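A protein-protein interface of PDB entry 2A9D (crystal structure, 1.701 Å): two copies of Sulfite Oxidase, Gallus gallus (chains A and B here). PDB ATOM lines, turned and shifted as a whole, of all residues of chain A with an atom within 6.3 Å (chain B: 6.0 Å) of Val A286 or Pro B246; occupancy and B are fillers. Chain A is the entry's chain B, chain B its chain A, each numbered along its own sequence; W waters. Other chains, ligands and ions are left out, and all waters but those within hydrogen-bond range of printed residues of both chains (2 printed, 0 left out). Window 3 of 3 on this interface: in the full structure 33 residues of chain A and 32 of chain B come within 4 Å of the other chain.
Val A286 touches just one residue of chain B: Pro B246. Of chain A, only Val A286 and Tyr A342 come within 4 Å of Pro B246. Printed residues of chain A within 4 Å of Ile B248: Tyr A342. Of the printed residues of chain B, Arg A287 touches Gly B230 (3.9996 Å). Of the printed residues of chain A, Gly B230 touches Arg A287 and Tyr A342. Of the printed residues of chain A, Ala B245 touches Tyr A342 (3.7 Å). Printed residues of chain B within 4 Å of Tyr A342: Lys B229 (3.9 Å), Gly B230 (3.1 Å), Ala B245 (3.7 Å), Pro B246 (2.6 Å) and Ile B248 (3.7 Å). The nearest residue of chain B that does not touch Val A286 is Thr B244 (4.8 Å). The nearest residue of chain A that does not touch Pro B246 is Glu A284 (5.0 Å). The nearest printed residue of chain A that does not touch Gly B230 is Val A286 (6.3 Å).
The backbone carbonyl oxygen of Tyr B228 sits at hydrogen-bond distance from the backbone NH of Ile B248 (3.0 Å). NZ of Lys B229 is in hydrogen-bond range of O of Tyr B242 (2.7 Å). NZ of Lys B229 lies within hydrogen-bond range of O of Ala B245 (2.8 Å). N of Val A286 is in hydrogen-bond range of O of Val A338 (2.8 Å). OD1 of Asp A339 lies within hydrogen-bond range of N of Tyr A342, at 3.2 Å.
No position is printed for both chains. Of the 7 pairs that touch across the chains among the printed residues, none has its exchanged pair printed and touching as well.
N of Gly B230 lies within hydrogen-bond range of OH of Tyr A342. The side-chain hydroxyl (OH) of Tyr A342 lies within hydrogen-bond range of the backbone carbonyl oxygen (O) of Pro B246 (2.6 Å).
Water W1 lies within hydrogen-bond range of the backbone carbonyl oxygen (O) of Gly B230 and the guanidinium group (NH1) of Arg A287. Water W2 bridges O of Thr B244 and O of Val A286.
Of the 11 printed residues of chain A, 3 touch a printed residue of chain B. Hydrophobic or aromatic side chains of chain A that line the printed part of chain B: Val A286 and Tyr A342. Along chain A the printed residues that touch a printed residue of chain B span positions 286 to 342. Of the 10 printed residues of chain B, 5 touch a printed residue of chain A. Hydrophobic or aromatic side chains of chain B that line the printed part of chain A: Ala B245, Pro B246 and Ile B248. Among the printed residues, 7 pairs touch across the chains. Among the printed residues, no Asp or Glu carboxylate lies within 4 Å of a Lys or Arg side-chain nitrogen of the other chain.
Among the printed residues, pairs that only touch across the chains: Tyr A342 with Ile B248, Tyr A342 with Ala B245, Val A286 with Pro B246, Tyr A342 with Lys B229 and Arg A287 with Gly B230.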
ATOM      1  N   GLU A 284     -23.556 -12.487   0.330  1.00  0.00           N
ATOM      2  CA  GLU A 284     -23.410 -13.752   1.067  1.00  0.00           C
ATOM      3  C   GLU A 284     -22.913 -14.875   0.160  1.00  0.00           C
ATOM      4  O   GLU A 284     -23.034 -14.825  -1.062  1.00  0.00           O
ATOM      5  CB  GLU A 284     -24.716 -14.179   1.738  1.00  0.00           C
ATOM      6  CG  GLU A 284     -25.773 -14.558   0.764  1.00  0.00           C
ATOM      7  CD  GLU A 284     -26.943 -15.361   1.376  1.00  0.00           C
ATOM      8  OE1 GLU A 284     -26.997 -15.569   2.615  1.00  0.00           O
ATOM      9  OE2 GLU A 284     -27.794 -15.812   0.575  1.00  0.00           O
ATOM     10  N   VAL A 285     -22.285 -15.868   0.775  1.00  0.00           N
ATOM     11  CA  VAL A 285     -21.906 -17.077   0.084  1.00  0.00           C
ATOM     12  C   VAL A 285     -23.158 -17.954   0.066  1.00  0.00           C
ATOM     13  O   VAL A 285     -23.736 -18.255   1.141  1.00  0.00           O
ATOM     14  CB  VAL A 285     -20.793 -17.794   0.843  1.00  0.00           C
ATOM     15  CG1 VAL A 285     -20.543 -19.155   0.230  1.00  0.00           C
ATOM     16  CG2 VAL A 285     -19.527 -16.944   0.847  1.00  0.00           C
ATOM     17  N   VAL A 286     -23.615 -18.307  -1.132  1.00  0.00           N
ATOM     18  CA  VAL A 286     -24.863 -19.087  -1.288  1.00  0.00           C
ATOM     19  C   VAL A 286     -24.599 -20.592  -1.467  1.00  0.00           C
ATOM     20  O   VAL A 286     -25.493 -21.410  -1.263  1.00  0.00           O
ATOM     21  CB  VAL A 286     -25.778 -18.537  -2.388  1.00  0.00           C
ATOM     22  CG1 VAL A 286     -26.013 -17.068  -2.129  1.00  0.00           C
ATOM     23  CG2 VAL A 286     -25.246 -18.789  -3.755  1.00  0.00           C
ATOM     24  N   ARG A 287     -23.369 -20.940  -1.807  1.00  0.00           N
ATOM     25  CA  ARG A 287     -23.002 -22.331  -1.984  1.00  0.00           C
ATOM     26  C   ARG A 287     -21.497 -22.476  -2.029  1.00  0.00           C
ATOM     27  O   ARG A 287     -20.792 -21.572  -2.495  1.00  0.00           O
ATOM     28  CB  ARG A 287     -23.583 -22.863  -3.309  1.00  0.00           C
ATOM     29  CG  ARG A 287     -23.610 -24.386  -3.400  1.00  0.00           C
ATOM     30  CD  ARG A 287     -24.192 -24.939  -4.664  1.00  0.00           C
ATOM     31  NE  ARG A 287     -23.311 -24.779  -5.831  1.00  0.00           N
ATOM     32  CZ  ARG A 287     -23.460 -23.902  -6.813  1.00  0.00           C
ATOM     33  NH1 ARG A 287     -24.485 -23.078  -6.871  1.00  0.00           N
ATOM     34  NH2 ARG A 287     -22.578 -23.893  -7.795  1.00  0.00           N
ATOM     35  N   VAL A 288     -21.019 -23.639  -1.592  1.00  0.00           N
ATOM     36  CA  VAL A 288     -19.627 -24.050  -1.746  1.00  0.00           C
ATOM     37  C   VAL A 288     -19.626 -25.478  -2.300  1.00  0.00           C
ATOM     38  O   VAL A 288     -20.259 -26.373  -1.724  1.00  0.00           O
ATOM     39  CB  VAL A 288     -18.837 -24.021  -0.418  1.00  0.00           C
ATOM     40  CG1 VAL A 288     -17.428 -24.589  -0.640  1.00  0.00           C
ATOM     41  CG2 VAL A 288     -18.777 -22.588   0.135  1.00  0.00           C
ATOM     42  N   LEU A 303     -22.878 -25.257   4.903  1.00  0.00           N
ATOM     43  CA  LEU A 303     -22.482 -23.939   5.333  1.00  0.00           C
ATOM     44  C   LEU A 303     -22.848 -23.771   6.804  1.00  0.00           C
ATOM     45  O   LEU A 303     -23.992 -23.976   7.204  1.00  0.00           O
ATOM     46  CB  LEU A 303     -23.139 -22.846   4.489  1.00  0.00           C
ATOM     47  CG  LEU A 303     -22.879 -22.973   2.984  1.00  0.00           C
ATOM     48  CD1 LEU A 303     -23.582 -21.851   2.183  1.00  0.00           C
ATOM     49  CD2 LEU A 303     -21.408 -23.004   2.646  1.00  0.00           C
ATOM     50  N   VAL A 338     -19.833 -19.607  -4.412  1.00  0.00           N
ATOM     51  CA  VAL A 338     -20.755 -18.789  -5.252  1.00  0.00           C
ATOM     52  C   VAL A 338     -21.432 -17.772  -4.344  1.00  0.00           C
ATOM     53  O   VAL A 338     -21.857 -18.124  -3.258  1.00  0.00           O
ATOM     54  CB  VAL A 338     -21.837 -19.691  -5.917  1.00  0.00           C
ATOM     55  CG1 VAL A 338     -22.733 -18.883  -6.801  1.00  0.00           C
ATOM     56  CG2 VAL A 338     -21.184 -20.861  -6.679  1.00  0.00           C
ATOM     57  N   ASP A 339     -21.509 -16.503  -4.752  1.00  0.00           N
ATOM     58  CA  ASP A 339     -22.070 -15.480  -3.869  1.00  0.00           C
ATOM     59  C   ASP A 339     -23.489 -15.105  -4.316  1.00  0.00           C
ATOM     60  O   ASP A 339     -24.019 -15.662  -5.281  1.00  0.00           O
ATOM     61  CB  ASP A 339     -21.134 -14.273  -3.687  1.00  0.00           C
ATOM     62  CG  ASP A 339     -21.067 -13.328  -4.889  1.00  0.00           C
ATOM     63  OD1 ASP A 339     -21.917 -13.399  -5.802  1.00  0.00           O
ATOM     64  OD2 ASP A 339     -20.147 -12.454  -4.876  1.00  0.00           O
ATOM     65  N   SER A 340     -24.061 -14.128  -3.639  1.00  0.00           N
ATOM     66  CA  SER A 340     -25.444 -13.753  -3.887  1.00  0.00           C
ATOM     67  C   SER A 340     -25.717 -13.117  -5.238  1.00  0.00           C
ATOM     68  O   SER A 340     -26.877 -13.024  -5.622  1.00  0.00           O
ATOM     69  CB  SER A 340     -25.962 -12.868  -2.772  1.00  0.00           C
ATOM     70  OG  SER A 340     -25.122 -11.791  -2.568  1.00  0.00           O
ATOM     71  N   SER A 341     -24.684 -12.617  -5.913  1.00  0.00           N
ATOM     72  CA  SER A 341     -24.839 -12.118  -7.266  1.00  0.00           C
ATOM     73  C   SER A 341     -24.369 -13.200  -8.273  1.00  0.00           C
ATOM     74  O   SER A 341     -24.235 -12.930  -9.479  1.00  0.00           O
ATOM     75  CB  SER A 341     -24.044 -10.843  -7.375  1.00  0.00           C
ATOM     76  OG  SER A 341     -23.742 -10.470  -8.710  1.00  0.00           O
ATOM     77  N   TYR A 342     -24.247 -14.438  -7.791  1.00  0.00           N
ATOM     78  CA  TYR A 342     -23.822 -15.595  -8.564  1.00  0.00           C
ATOM     79  C   TYR A 342     -22.445 -15.409  -9.238  1.00  0.00           C
ATOM     80  O   TYR A 342     -22.166 -15.993 -10.278  1.00  0.00           O
ATOM     81  CB  TYR A 342     -24.886 -16.052  -9.545  1.00  0.00           C
ATOM     82  CG  TYR A 342     -26.017 -16.815  -8.888  1.00  0.00           C
ATOM     83  CD1 TYR A 342     -25.861 -18.149  -8.553  1.00  0.00           C
ATOM     84  CD2 TYR A 342     -27.206 -16.174  -8.540  1.00  0.00           C
ATOM     85  CE1 TYR A 342     -26.888 -18.855  -7.945  1.00  0.00           C
ATOM     86  CE2 TYR A 342     -28.267 -16.880  -7.969  1.00  0.00           C
ATOM     87  CZ  TYR A 342     -28.101 -18.213  -7.675  1.00  0.00           C
ATOM     88  OH  TYR A 342     -29.164 -18.969  -7.126  1.00  0.00           O
ATOM     89  N   GLU B 218     -41.238 -12.839  -1.027  1.00  0.00           N
ATOM     90  CA  GLU B 218     -41.002 -12.816  -2.462  1.00  0.00           C
ATOM     91  C   GLU B 218     -42.254 -13.129  -3.237  1.00  0.00           C
ATOM     92  O   GLU B 218     -43.182 -13.757  -2.724  1.00  0.00           O
ATOM     93  CB  GLU B 218     -40.030 -13.901  -2.880  1.00  0.00           C
ATOM     94  CG  GLU B 218     -38.600 -13.604  -2.726  1.00  0.00           C
ATOM     95  CD  GLU B 218     -37.775 -14.710  -3.369  1.00  0.00           C
ATOM     96  OE1 GLU B 218     -37.967 -15.900  -3.023  1.00  0.00           O
ATOM     97  OE2 GLU B 218     -36.965 -14.375  -4.233  1.00  0.00           O
ATOM     98  N   TYR B 228     -35.128 -19.868 -12.665  1.00  0.00           N
ATOM     99  CA  TYR B 228     -34.082 -18.851 -12.582  1.00  0.00           C
ATOM    100  C   TYR B 228     -33.286 -18.830 -11.266  1.00  0.00           C
ATOM    101  O   TYR B 228     -33.202 -17.835 -10.561  1.00  0.00           O
ATOM    102  CB  TYR B 228     -34.708 -17.477 -12.869  1.00  0.00           C
ATOM    103  CG  TYR B 228     -35.379 -17.428 -14.213  1.00  0.00           C
ATOM    104  CD1 TYR B 228     -34.660 -17.707 -15.366  1.00  0.00           C
ATOM    105  CD2 TYR B 228     -36.755 -17.150 -14.333  1.00  0.00           C
ATOM    106  CE1 TYR B 228     -35.247 -17.655 -16.592  1.00  0.00           C
ATOM    107  CE2 TYR B 228     -37.358 -17.137 -15.548  1.00  0.00           C
ATOM    108  CZ  TYR B 228     -36.603 -17.369 -16.686  1.00  0.00           C
ATOM    109  OH  TYR B 228     -37.206 -17.310 -17.927  1.00  0.00           O
ATOM    110  N   LYS B 229     -32.662 -19.965 -10.973  1.00  0.00           N
ATOM    111  CA  LYS B 229     -31.738 -20.073  -9.872  1.00  0.00           C
ATOM    112  C   LYS B 229     -30.543 -20.885 -10.351  1.00  0.00           C
ATOM    113  O   LYS B 229     -30.632 -21.577 -11.342  1.00  0.00           O
ATOM    114  CB  LYS B 229     -32.408 -20.750  -8.672  1.00  0.00           C
ATOM    115  CG  LYS B 229     -33.607 -20.029  -8.139  1.00  0.00           C
ATOM    116  CD  LYS B 229     -34.064 -20.554  -6.779  1.00  0.00           C
ATOM    117  CE  LYS B 229     -35.220 -19.740  -6.196  1.00  0.00           C
ATOM    118  NZ  LYS B 229     -35.519 -20.164  -4.797  1.00  0.00           N
ATOM    119  N   GLY B 230     -29.418 -20.762  -9.646  1.00  0.00           N
ATOM    120  CA  GLY B 230     -28.204 -21.520  -9.926  1.00  0.00           C
ATOM    121  C   GLY B 230     -28.022 -22.664  -8.954  1.00  0.00           C
ATOM    122  O   GLY B 230     -28.341 -22.519  -7.774  1.00  0.00           O
ATOM    123  N   TYR B 242     -35.586 -26.122  -5.586  1.00  0.00           N
ATOM    124  CA  TYR B 242     -35.493 -24.683  -5.730  1.00  0.00           C
ATOM    125  C   TYR B 242     -35.480 -23.913  -4.420  1.00  0.00           C
ATOM    126  O   TYR B 242     -35.071 -22.760  -4.398  1.00  0.00           O
ATOM    127  CB  TYR B 242     -36.581 -24.139  -6.683  1.00  0.00           C
ATOM    128  CG  TYR B 242     -36.141 -24.178  -8.134  1.00  0.00           C
ATOM    129  CD1 TYR B 242     -36.137 -25.360  -8.841  1.00  0.00           C
ATOM    130  CD2 TYR B 242     -35.636 -23.037  -8.770  1.00  0.00           C
ATOM    131  CE1 TYR B 242     -35.723 -25.397 -10.183  1.00  0.00           C
ATOM    132  CE2 TYR B 242     -35.219 -23.059 -10.106  1.00  0.00           C
ATOM    133  CZ  TYR B 242     -35.247 -24.243 -10.801  1.00  0.00           C
ATOM    134  OH  TYR B 242     -34.826 -24.270 -12.122  1.00  0.00           O
ATOM    135  N   THR B 244     -33.307 -24.461  -2.211  1.00  0.00           N
ATOM    136  CA  THR B 244     -31.921 -24.464  -1.725  1.00  0.00           C
ATOM    137  C   THR B 244     -31.050 -23.356  -2.312  1.00  0.00           C
ATOM    138  O   THR B 244     -29.866 -23.284  -1.992  1.00  0.00           O
ATOM    139  CB  THR B 244     -31.215 -25.819  -2.013  1.00  0.00           C
ATOM    140  OG1 THR B 244     -31.008 -25.962  -3.431  1.00  0.00           O
ATOM    141  CG2 THR B 244     -32.011 -27.003  -1.449  1.00  0.00           C
ATOM    142  N   ALA B 245     -31.621 -22.488  -3.136  1.00  0.00           N
ATOM    143  CA  ALA B 245     -30.840 -21.429  -3.799  1.00  0.00           C
ATOM    144  C   ALA B 245     -31.658 -20.152  -3.871  1.00  0.00           C
ATOM    145  O   ALA B 245     -32.889 -20.195  -3.810  1.00  0.00           O
ATOM    146  CB  ALA B 245     -30.462 -21.866  -5.190  1.00  0.00           C
ATOM    147  N   PRO B 246     -30.978 -19.015  -3.988  1.00  0.00           N
ATOM    148  CA  PRO B 246     -31.656 -17.736  -4.105  1.00  0.00           C
ATOM    149  C   PRO B 246     -32.069 -17.427  -5.536  1.00  0.00           C
ATOM    150  O   PRO B 246     -31.433 -17.850  -6.506  1.00  0.00           O
ATOM    151  CB  PRO B 246     -30.595 -16.742  -3.622  1.00  0.00           C
ATOM    152  CG  PRO B 246     -29.293 -17.406  -3.961  1.00  0.00           C
ATOM    153  CD  PRO B 246     -29.518 -18.874  -3.812  1.00  0.00           C
ATOM    154  N   ALA B 247     -33.163 -16.707  -5.658  1.00  0.00           N
ATOM    155  CA  ALA B 247     -33.583 -16.250  -6.958  1.00  0.00           C
ATOM    156  C   ALA B 247     -32.468 -15.417  -7.526  1.00  0.00           C
ATOM    157  O   ALA B 247     -31.962 -14.557  -6.827  1.00  0.00           O
ATOM    158  CB  ALA B 247     -34.815 -15.369  -6.785  1.00  0.00           C
ATOM    159  N   ILE B 248     -32.193 -15.571  -8.821  1.00  0.00           N
ATOM    160  CA  ILE B 248     -31.214 -14.710  -9.481  1.00  0.00           C
ATOM    161  C   ILE B 248     -31.749 -13.275  -9.456  1.00  0.00           C
ATOM    162  O   ILE B 248     -32.895 -13.042  -9.847  1.00  0.00           O
ATOM    163  CB  ILE B 248     -30.928 -15.124 -10.938  1.00  0.00           C
ATOM    164  CG1 ILE B 248     -30.265 -16.512 -11.025  1.00  0.00           C
ATOM    165  CG2 ILE B 248     -29.988 -14.082 -11.589  1.00  0.00           C
ATOM    166  CD1 ILE B 248     -30.356 -17.112 -12.409  1.00  0.00           C
HETATM  167  O   HOH W   1     -27.158 -23.184  -5.462  1.00  0.00           O
HETATM  168  O   HOH W   2     -27.605 -21.998  -3.016  1.00  0.00           O
